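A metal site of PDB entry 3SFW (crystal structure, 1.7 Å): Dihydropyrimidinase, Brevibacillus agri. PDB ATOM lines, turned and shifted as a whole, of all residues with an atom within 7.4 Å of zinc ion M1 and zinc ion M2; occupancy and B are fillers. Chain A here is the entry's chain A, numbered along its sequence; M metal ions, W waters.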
ATOM      1  N   HIS A  58      29.999 -11.340   0.817  1.00  0.00           N
ATOM      2  CA  HIS A  58      28.856 -10.442   0.626  1.00  0.00           C
ATOM      3  C   HIS A  58      29.201  -9.254  -0.280  1.00  0.00           C
ATOM      4  O   HIS A  58      29.513  -8.166   0.209  1.00  0.00           O
ATOM      5  CB  HIS A  58      28.279 -10.002   1.973  1.00  0.00           C
ATOM      6  CG  HIS A  58      26.914  -9.393   1.880  1.00  0.00           C
ATOM      7  ND1 HIS A  58      25.990  -9.472   2.909  1.00  0.00           N
ATOM      8  CD2 HIS A  58      26.280  -8.765   0.850  1.00  0.00           C
ATOM      9  CE1 HIS A  58      24.862  -8.905   2.529  1.00  0.00           C
ATOM     10  NE2 HIS A  58      25.014  -8.465   1.283  1.00  0.00           N
ATOM     11  N   THR A  59      29.196  -9.489  -1.599  1.00  0.00           N
ATOM     12  CA  THR A  59      29.547  -8.385  -2.534  1.00  0.00           C
ATOM     13  C   THR A  59      28.484  -8.245  -3.626  1.00  0.00           C
ATOM     14  O   THR A  59      27.743  -9.183  -3.907  1.00  0.00           O
ATOM     15  CB  THR A  59      30.936  -8.577  -3.183  1.00  0.00           C
ATOM     16  OG1 THR A  59      30.946  -9.728  -4.035  1.00  0.00           O
ATOM     17  CG2 THR A  59      32.009  -8.825  -2.052  1.00  0.00           C
ATOM     18  N   HIS A  60      28.397  -7.046  -4.198  1.00  0.00           N
ATOM     19  CA  HIS A  60      27.450  -6.728  -5.257  1.00  0.00           C
ATOM     20  C   HIS A  60      28.177  -5.925  -6.348  1.00  0.00           C
ATOM     21  O   HIS A  60      27.967  -4.704  -6.506  1.00  0.00           O
ATOM     22  CB  HIS A  60      26.284  -5.881  -4.691  1.00  0.00           C
ATOM     23  CG  HIS A  60      25.508  -6.574  -3.624  1.00  0.00           C
ATOM     24  ND1 HIS A  60      24.585  -7.561  -3.917  1.00  0.00           N
ATOM     25  CD2 HIS A  60      25.543  -6.474  -2.282  1.00  0.00           C
ATOM     26  CE1 HIS A  60      24.024  -7.990  -2.784  1.00  0.00           C
ATOM     27  NE2 HIS A  60      24.618  -7.354  -1.776  1.00  0.00           N
ATOM     28  N   MET A  63      26.317  -4.432 -10.127  1.00  0.00           N
ATOM     29  CA  MET A  63      24.954  -4.852  -9.828  1.00  0.00           C
ATOM     30  C   MET A  63      23.964  -3.780 -10.305  1.00  0.00           C
ATOM     31  O   MET A  63      24.063  -2.627  -9.912  1.00  0.00           O
ATOM     32  CB  MET A  63      24.803  -4.981  -8.304  1.00  0.00           C
ATOM     33  CG  MET A  63      23.359  -5.393  -7.870  1.00  0.00           C
ATOM     34  SD  MET A  63      23.076  -4.807  -6.179  1.00  0.00           S
ATOM     35  CE  MET A  63      21.547  -5.543  -5.745  1.00  0.00           C
ATOM     36  N   PHE A  65      20.771  -1.824  -9.701  1.00  0.00           N
ATOM     37  CA  PHE A  65      19.989  -1.572  -8.444  1.00  0.00           C
ATOM     38  C   PHE A  65      19.811  -0.075  -8.258  1.00  0.00           C
ATOM     39  O   PHE A  65      20.647   0.701  -8.716  1.00  0.00           O
ATOM     40  CB  PHE A  65      20.761  -2.153  -7.231  1.00  0.00           C
ATOM     41  CG  PHE A  65      19.967  -2.219  -5.924  1.00  0.00           C
ATOM     42  CD1 PHE A  65      18.767  -2.936  -5.840  1.00  0.00           C
ATOM     43  CD2 PHE A  65      20.594  -1.829  -4.749  1.00  0.00           C
ATOM     44  CE1 PHE A  65      18.141  -3.129  -4.608  1.00  0.00           C
ATOM     45  CE2 PHE A  65      19.982  -2.009  -3.495  1.00  0.00           C
ATOM     46  CZ  PHE A  65      18.723  -2.645  -3.440  1.00  0.00           C
ATOM     47  N   PHE A  92      26.504 -11.839  -5.164  1.00  0.00           N
ATOM     48  CA  PHE A  92      25.104 -12.207  -5.417  1.00  0.00           C
ATOM     49  C   PHE A  92      24.657 -12.099  -6.877  1.00  0.00           C
ATOM     50  O   PHE A  92      24.377 -10.988  -7.389  1.00  0.00           O
ATOM     51  CB  PHE A  92      24.194 -11.365  -4.495  1.00  0.00           C
ATOM     52  CG  PHE A  92      24.307 -11.756  -3.047  1.00  0.00           C
ATOM     53  CD1 PHE A  92      25.160 -11.064  -2.181  1.00  0.00           C
ATOM     54  CD2 PHE A  92      23.564 -12.789  -2.550  1.00  0.00           C
ATOM     55  CE1 PHE A  92      25.278 -11.413  -0.868  1.00  0.00           C
ATOM     56  CE2 PHE A  92      23.690 -13.176  -1.219  1.00  0.00           C
ATOM     57  CZ  PHE A  92      24.578 -12.496  -0.370  1.00  0.00           C
ATOM     58  N   KCX A 150      19.886 -16.936  -1.957  1.00  0.00           N
ATOM     59  CA  KCX A 150      19.566 -15.710  -1.239  1.00  0.00           C
ATOM     60  CB  KCX A 150      20.420 -14.556  -1.866  1.00  0.00           C
ATOM     61  CG  KCX A 150      20.124 -13.100  -1.286  1.00  0.00           C
ATOM     62  CD  KCX A 150      20.443 -13.036   0.279  1.00  0.00           C
ATOM     63  CE  KCX A 150      20.385 -11.550   0.785  1.00  0.00           C
ATOM     64  NZ  KCX A 150      21.455 -10.735   0.144  1.00  0.00           N
ATOM     65  C   KCX A 150      18.075 -15.385  -1.416  1.00  0.00           C
ATOM     66  O   KCX A 150      17.593 -15.294  -2.564  1.00  0.00           O
ATOM     67  CX  KCX A 150      21.606  -9.426   0.386  1.00  0.00           C
ATOM     68  OQ1 KCX A 150      20.932  -8.907   1.280  1.00  0.00           O
ATOM     69  OQ2 KCX A 150      22.459  -8.776  -0.265  1.00  0.00           O
ATOM     70  N   PHE A 152      15.365 -12.374  -0.446  1.00  0.00           N
ATOM     71  CA  PHE A 152      15.206 -11.026   0.079  1.00  0.00           C
ATOM     72  C   PHE A 152      13.814 -10.882   0.703  1.00  0.00           C
ATOM     73  O   PHE A 152      12.841 -11.235   0.092  1.00  0.00           O
ATOM     74  CB  PHE A 152      15.370 -10.008  -1.090  1.00  0.00           C
ATOM     75  CG  PHE A 152      16.778  -9.906  -1.597  1.00  0.00           C
ATOM     76  CD1 PHE A 152      17.190 -10.644  -2.726  1.00  0.00           C
ATOM     77  CD2 PHE A 152      17.688  -9.052  -0.994  1.00  0.00           C
ATOM     78  CE1 PHE A 152      18.477 -10.579  -3.197  1.00  0.00           C
ATOM     79  CE2 PHE A 152      18.975  -8.927  -1.502  1.00  0.00           C
ATOM     80  CZ  PHE A 152      19.387  -9.725  -2.594  1.00  0.00           C
ATOM     81  N   TYR A 155      12.599  -4.917   0.138  1.00  0.00           N
ATOM     82  CA  TYR A 155      12.625  -4.383  -1.253  1.00  0.00           C
ATOM     83  C   TYR A 155      11.401  -4.815  -2.045  1.00  0.00           C
ATOM     84  O   TYR A 155      11.493  -5.398  -3.120  1.00  0.00           O
ATOM     85  CB  TYR A 155      13.927  -4.791  -1.969  1.00  0.00           C
ATOM     86  CG  TYR A 155      15.191  -4.408  -1.230  1.00  0.00           C
ATOM     87  CD1 TYR A 155      15.543  -3.076  -0.994  1.00  0.00           C
ATOM     88  CD2 TYR A 155      16.066  -5.395  -0.804  1.00  0.00           C
ATOM     89  CE1 TYR A 155      16.749  -2.760  -0.309  1.00  0.00           C
ATOM     90  CE2 TYR A 155      17.258  -5.091  -0.140  1.00  0.00           C
ATOM     91  CZ  TYR A 155      17.582  -3.794   0.108  1.00  0.00           C
ATOM     92  OH  TYR A 155      18.796  -3.535   0.727  1.00  0.00           O
ATOM     93  N   LEU A 159      12.983  -6.903  -5.225  1.00  0.00           N
ATOM     94  CA  LEU A 159      13.695  -8.185  -4.928  1.00  0.00           C
ATOM     95  C   LEU A 159      12.891  -9.083  -4.004  1.00  0.00           C
ATOM     96  O   LEU A 159      13.172 -10.270  -3.887  1.00  0.00           O
ATOM     97  CB  LEU A 159      15.092  -7.923  -4.291  1.00  0.00           C
ATOM     98  CG  LEU A 159      16.066  -6.983  -5.011  1.00  0.00           C
ATOM     99  CD1 LEU A 159      17.383  -6.860  -4.196  1.00  0.00           C
ATOM    100  CD2 LEU A 159      16.352  -7.514  -6.450  1.00  0.00           C
ATOM    101  N   VAL A 182      19.253 -15.039   4.127  1.00  0.00           N
ATOM    102  CA  VAL A 182      18.188 -14.046   4.036  1.00  0.00           C
ATOM    103  C   VAL A 182      18.688 -12.629   4.264  1.00  0.00           C
ATOM    104  O   VAL A 182      19.399 -12.394   5.210  1.00  0.00           O
ATOM    105  CB  VAL A 182      17.053 -14.366   5.040  1.00  0.00           C
ATOM    106  CG1 VAL A 182      16.220 -13.204   5.292  1.00  0.00           C
ATOM    107  CG2 VAL A 182      16.234 -15.565   4.549  1.00  0.00           C
ATOM    108  N   HIS A 183      18.103 -11.688   3.516  1.00  0.00           N
ATOM    109  CA  HIS A 183      18.058 -10.261   3.896  1.00  0.00           C
ATOM    110  C   HIS A 183      16.775 -10.109   4.738  1.00  0.00           C
ATOM    111  O   HIS A 183      15.668 -10.148   4.179  1.00  0.00           O
ATOM    112  CB  HIS A 183      17.976  -9.340   2.638  1.00  0.00           C
ATOM    113  CG  HIS A 183      17.793  -7.888   2.981  1.00  0.00           C
ATOM    114  ND1 HIS A 183      18.722  -6.911   2.661  1.00  0.00           N
ATOM    115  CD2 HIS A 183      16.802  -7.256   3.656  1.00  0.00           C
ATOM    116  CE1 HIS A 183      18.284  -5.734   3.097  1.00  0.00           C
ATOM    117  NE2 HIS A 183      17.130  -5.919   3.724  1.00  0.00           N
ATOM    118  N   ALA A 184      16.932  -9.942   6.053  1.00  0.00           N
ATOM    119  CA  ALA A 184      15.770 -10.073   6.958  1.00  0.00           C
ATOM    120  C   ALA A 184      15.325  -8.685   7.441  1.00  0.00           C
ATOM    121  O   ALA A 184      15.680  -8.257   8.557  1.00  0.00           O
ATOM    122  CB  ALA A 184      16.100 -10.996   8.183  1.00  0.00           C
ATOM    123  N   GLU A 185      14.461  -8.036   6.678  1.00  0.00           N
ATOM    124  CA  GLU A 185      13.631  -6.912   7.220  1.00  0.00           C
ATOM    125  C   GLU A 185      12.234  -7.172   6.697  1.00  0.00           C
ATOM    126  O   GLU A 185      12.080  -7.625   5.537  1.00  0.00           O
ATOM    127  CB  GLU A 185      14.067  -5.547   6.670  1.00  0.00           C
ATOM    128  CG  GLU A 185      15.519  -5.116   7.013  1.00  0.00           C
ATOM    129  CD  GLU A 185      15.876  -3.837   6.310  1.00  0.00           C
ATOM    130  OE1 GLU A 185      16.098  -3.875   5.053  1.00  0.00           O
ATOM    131  OE2 GLU A 185      15.817  -2.770   6.997  1.00  0.00           O
ATOM    132  N   VAL A 238      22.181 -12.530   6.649  1.00  0.00           N
ATOM    133  CA  VAL A 238      23.245 -11.607   6.213  1.00  0.00           C
ATOM    134  C   VAL A 238      23.041 -10.279   6.963  1.00  0.00           C
ATOM    135  O   VAL A 238      21.969 -10.028   7.515  1.00  0.00           O
ATOM    136  CB  VAL A 238      23.230 -11.302   4.666  1.00  0.00           C
ATOM    137  CG1 VAL A 238      23.287 -12.616   3.845  1.00  0.00           C
ATOM    138  CG2 VAL A 238      21.953 -10.526   4.277  1.00  0.00           C
ATOM    139  N   HIS A 239      24.119  -9.487   7.030  1.00  0.00           N
ATOM    140  CA  HIS A 239      24.104  -8.170   7.678  1.00  0.00           C
ATOM    141  C   HIS A 239      23.154  -8.072   8.874  1.00  0.00           C
ATOM    142  O   HIS A 239      22.242  -7.250   8.871  1.00  0.00           O
ATOM    143  CB  HIS A 239      23.875  -6.985   6.664  1.00  0.00           C
ATOM    144  CG  HIS A 239      22.696  -7.140   5.727  1.00  0.00           C
ATOM    145  ND1 HIS A 239      21.422  -7.474   6.153  1.00  0.00           N
ATOM    146  CD2 HIS A 239      22.596  -6.860   4.396  1.00  0.00           C
ATOM    147  CE1 HIS A 239      20.596  -7.463   5.105  1.00  0.00           C
ATOM    148  NE2 HIS A 239      21.282  -7.082   4.043  1.00  0.00           N
ATOM    149  N   GLU A 262      25.915 -13.173  10.016  1.00  0.00           N
ATOM    150  CA  GLU A 262      26.991 -12.349   9.500  1.00  0.00           C
ATOM    151  C   GLU A 262      26.771 -10.934  10.025  1.00  0.00           C
ATOM    152  O   GLU A 262      25.629 -10.485  10.129  1.00  0.00           O
ATOM    153  CB  GLU A 262      26.793 -12.282   7.983  1.00  0.00           C
ATOM    154  CG  GLU A 262      27.779 -11.415   7.213  1.00  0.00           C
ATOM    155  CD  GLU A 262      27.296 -11.315   5.754  1.00  0.00           C
ATOM    156  OE1 GLU A 262      26.485 -10.394   5.450  1.00  0.00           O
ATOM    157  OE2 GLU A 262      27.659 -12.218   4.953  1.00  0.00           O
ATOM    158  N   TYR A 267      28.146  -1.691  10.530  1.00  0.00           N
ATOM    159  CA  TYR A 267      27.258  -1.807  11.701  1.00  0.00           C
ATOM    160  C   TYR A 267      28.057  -1.891  12.995  1.00  0.00           C
ATOM    161  O   TYR A 267      27.499  -1.713  14.048  1.00  0.00           O
ATOM    162  CB  TYR A 267      26.289  -2.995  11.554  1.00  0.00           C
ATOM    163  CG  TYR A 267      25.494  -2.902  10.263  1.00  0.00           C
ATOM    164  CD1 TYR A 267      25.679  -3.830   9.233  1.00  0.00           C
ATOM    165  CD2 TYR A 267      24.577  -1.842  10.079  1.00  0.00           C
ATOM    166  CE1 TYR A 267      24.996  -3.728   8.022  1.00  0.00           C
ATOM    167  CE2 TYR A 267      23.856  -1.750   8.891  1.00  0.00           C
ATOM    168  CZ  TYR A 267      24.053  -2.684   7.866  1.00  0.00           C
ATOM    169  OH  TYR A 267      23.313  -2.566   6.694  1.00  0.00           O
ATOM    170  N   SER A 288      20.914  -0.711   3.593  1.00  0.00           N
ATOM    171  CA  SER A 288      19.841  -1.353   4.380  1.00  0.00           C
ATOM    172  C   SER A 288      20.347  -2.703   4.839  1.00  0.00           C
ATOM    173  O   SER A 288      21.102  -3.315   4.119  1.00  0.00           O
ATOM    174  CB  SER A 288      18.609  -1.584   3.497  1.00  0.00           C
ATOM    175  OG  SER A 288      18.100  -0.331   3.042  1.00  0.00           O
ATOM    176  N   PRO A 289      20.001  -3.130   6.054  1.00  0.00           N
ATOM    177  CA  PRO A 289      19.327  -2.378   7.112  1.00  0.00           C
ATOM    178  C   PRO A 289      20.066  -1.132   7.436  1.00  0.00           C
ATOM    179  O   PRO A 289      21.249  -1.005   7.160  1.00  0.00           O
ATOM    180  CB  PRO A 289      19.352  -3.323   8.317  1.00  0.00           C
ATOM    181  CG  PRO A 289      20.482  -4.277   8.024  1.00  0.00           C
ATOM    182  CD  PRO A 289      20.446  -4.462   6.543  1.00  0.00           C
ATOM    183  N   SER A 314      31.171  -7.544   3.706  1.00  0.00           N
ATOM    184  CA  SER A 314      31.142  -6.063   3.525  1.00  0.00           C
ATOM    185  C   SER A 314      29.737  -5.559   3.112  1.00  0.00           C
ATOM    186  O   SER A 314      29.385  -4.424   3.467  1.00  0.00           O
ATOM    187  CB  SER A 314      32.156  -5.611   2.455  1.00  0.00           C
ATOM    188  OG  SER A 314      31.862  -6.247   1.215  1.00  0.00           O
ATOM    189  N   ASP A 315      28.969  -6.364   2.345  1.00  0.00           N
ATOM    190  CA  ASP A 315      27.789  -5.825   1.595  1.00  0.00           C
ATOM    191  C   ASP A 315      28.277  -4.651   0.706  1.00  0.00           C
ATOM    192  O   ASP A 315      27.617  -3.589   0.576  1.00  0.00           O
ATOM    193  CB  ASP A 315      26.583  -5.408   2.501  1.00  0.00           C
ATOM    194  CG  ASP A 315      25.286  -5.201   1.737  1.00  0.00           C
ATOM    195  OD1 ASP A 315      25.160  -5.744   0.594  1.00  0.00           O
ATOM    196  OD2 ASP A 315      24.395  -4.464   2.270  1.00  0.00           O
ATOM    197  N   HIS A 316      29.408  -4.865   0.063  1.00  0.00           N
ATOM    198  CA  HIS A 316      29.960  -3.812  -0.834  1.00  0.00           C
ATOM    199  C   HIS A 316      28.952  -3.578  -1.963  1.00  0.00           C
ATOM    200  O   HIS A 316      28.662  -4.473  -2.759  1.00  0.00           O
ATOM    201  CB  HIS A 316      31.275  -4.294  -1.456  1.00  0.00           C
ATOM    202  CG  HIS A 316      31.960  -3.240  -2.271  1.00  0.00           C
ATOM    203  ND1 HIS A 316      32.389  -2.055  -1.719  1.00  0.00           N
ATOM    204  CD2 HIS A 316      32.296  -3.206  -3.574  1.00  0.00           C
ATOM    205  CE1 HIS A 316      32.956  -1.314  -2.654  1.00  0.00           C
ATOM    206  NE2 HIS A 316      32.903  -1.992  -3.802  1.00  0.00           N
ATOM    207  N   CYS A 317      28.438  -2.349  -2.064  1.00  0.00           N
ATOM    208  CA  CYS A 317      27.357  -2.086  -3.008  1.00  0.00           C
ATOM    209  C   CYS A 317      27.480  -0.552  -3.334  1.00  0.00           C
ATOM    210  O   CYS A 317      26.622   0.241  -2.954  1.00  0.00           O
ATOM    211  CB  CYS A 317      26.015  -2.446  -2.328  1.00  0.00           C
ATOM    212  SG  CYS A 317      24.577  -2.477  -3.492  1.00  0.00           S
HETATM  213 ZN    ZN M   1      20.798  -6.926   1.917  1.00  0.00          ZN
HETATM  214 ZN    ZN M   2      23.702  -7.223   0.124  1.00  0.00          ZN
HETATM  215  O   HOH W   1      20.889  -4.687   1.849  1.00  0.00           O
HETATM  216  O   HOH W   2      20.380  -6.301  -0.053  1.00  0.00           O
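The backbone NH (N) of His 60 lies within hydrogen-bond range of the backbone carbonyl oxygen (O) of His 316 (3.0 Å). The backbone carbonyl oxygen (O) of His 58 lies within hydrogen-bond range of the backbone NH (N) of His 316 (3.3 Å). The side-chain carboxylate (OE1) of Glu 262 sits at hydrogen-bond distance from a ring nitrogen (ND1) of His 58 (2.7 Å). The side-chain hydroxyl (OG) of Ser 314 lies within hydrogen-bond range of the backbone carbonyl oxygen (O) of His 58. The backbone NH of His 239 is in hydrogen-bond range of the side-chain carboxylate of Glu 262, at 3.0 Å. The side-chain carboxylate of Glu 185 sits at hydrogen-bond distance from a ring nitrogen (NE2) of His 183 (2.6 Å).
Four residues have an atom within 4 Å of zinc ion M2: His 58, His 60, KCX 150 and Asp 315.
Zinc ion M1 is bound by OQ1 of KCX 150, water W2, NE2 of His 239, ND1 of His 183 and water W1. Zinc ion M1 has five donor atoms within binding distance.
Zinc ion M2 is bound by OQ2 of KCX 150 (2.0 Å), a ring nitrogen (NE2) of His 60 (2.1 Å), the side-chain carboxylate of Asp 315 (2.1 Å) and a ring nitrogen (NE2) of His 58 (2.1 Å). Zinc ion M2 has four donor atoms within binding distance.
Water W1 lies within hydrogen-bond range of OH of Tyr 155 and O of Ser 288.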
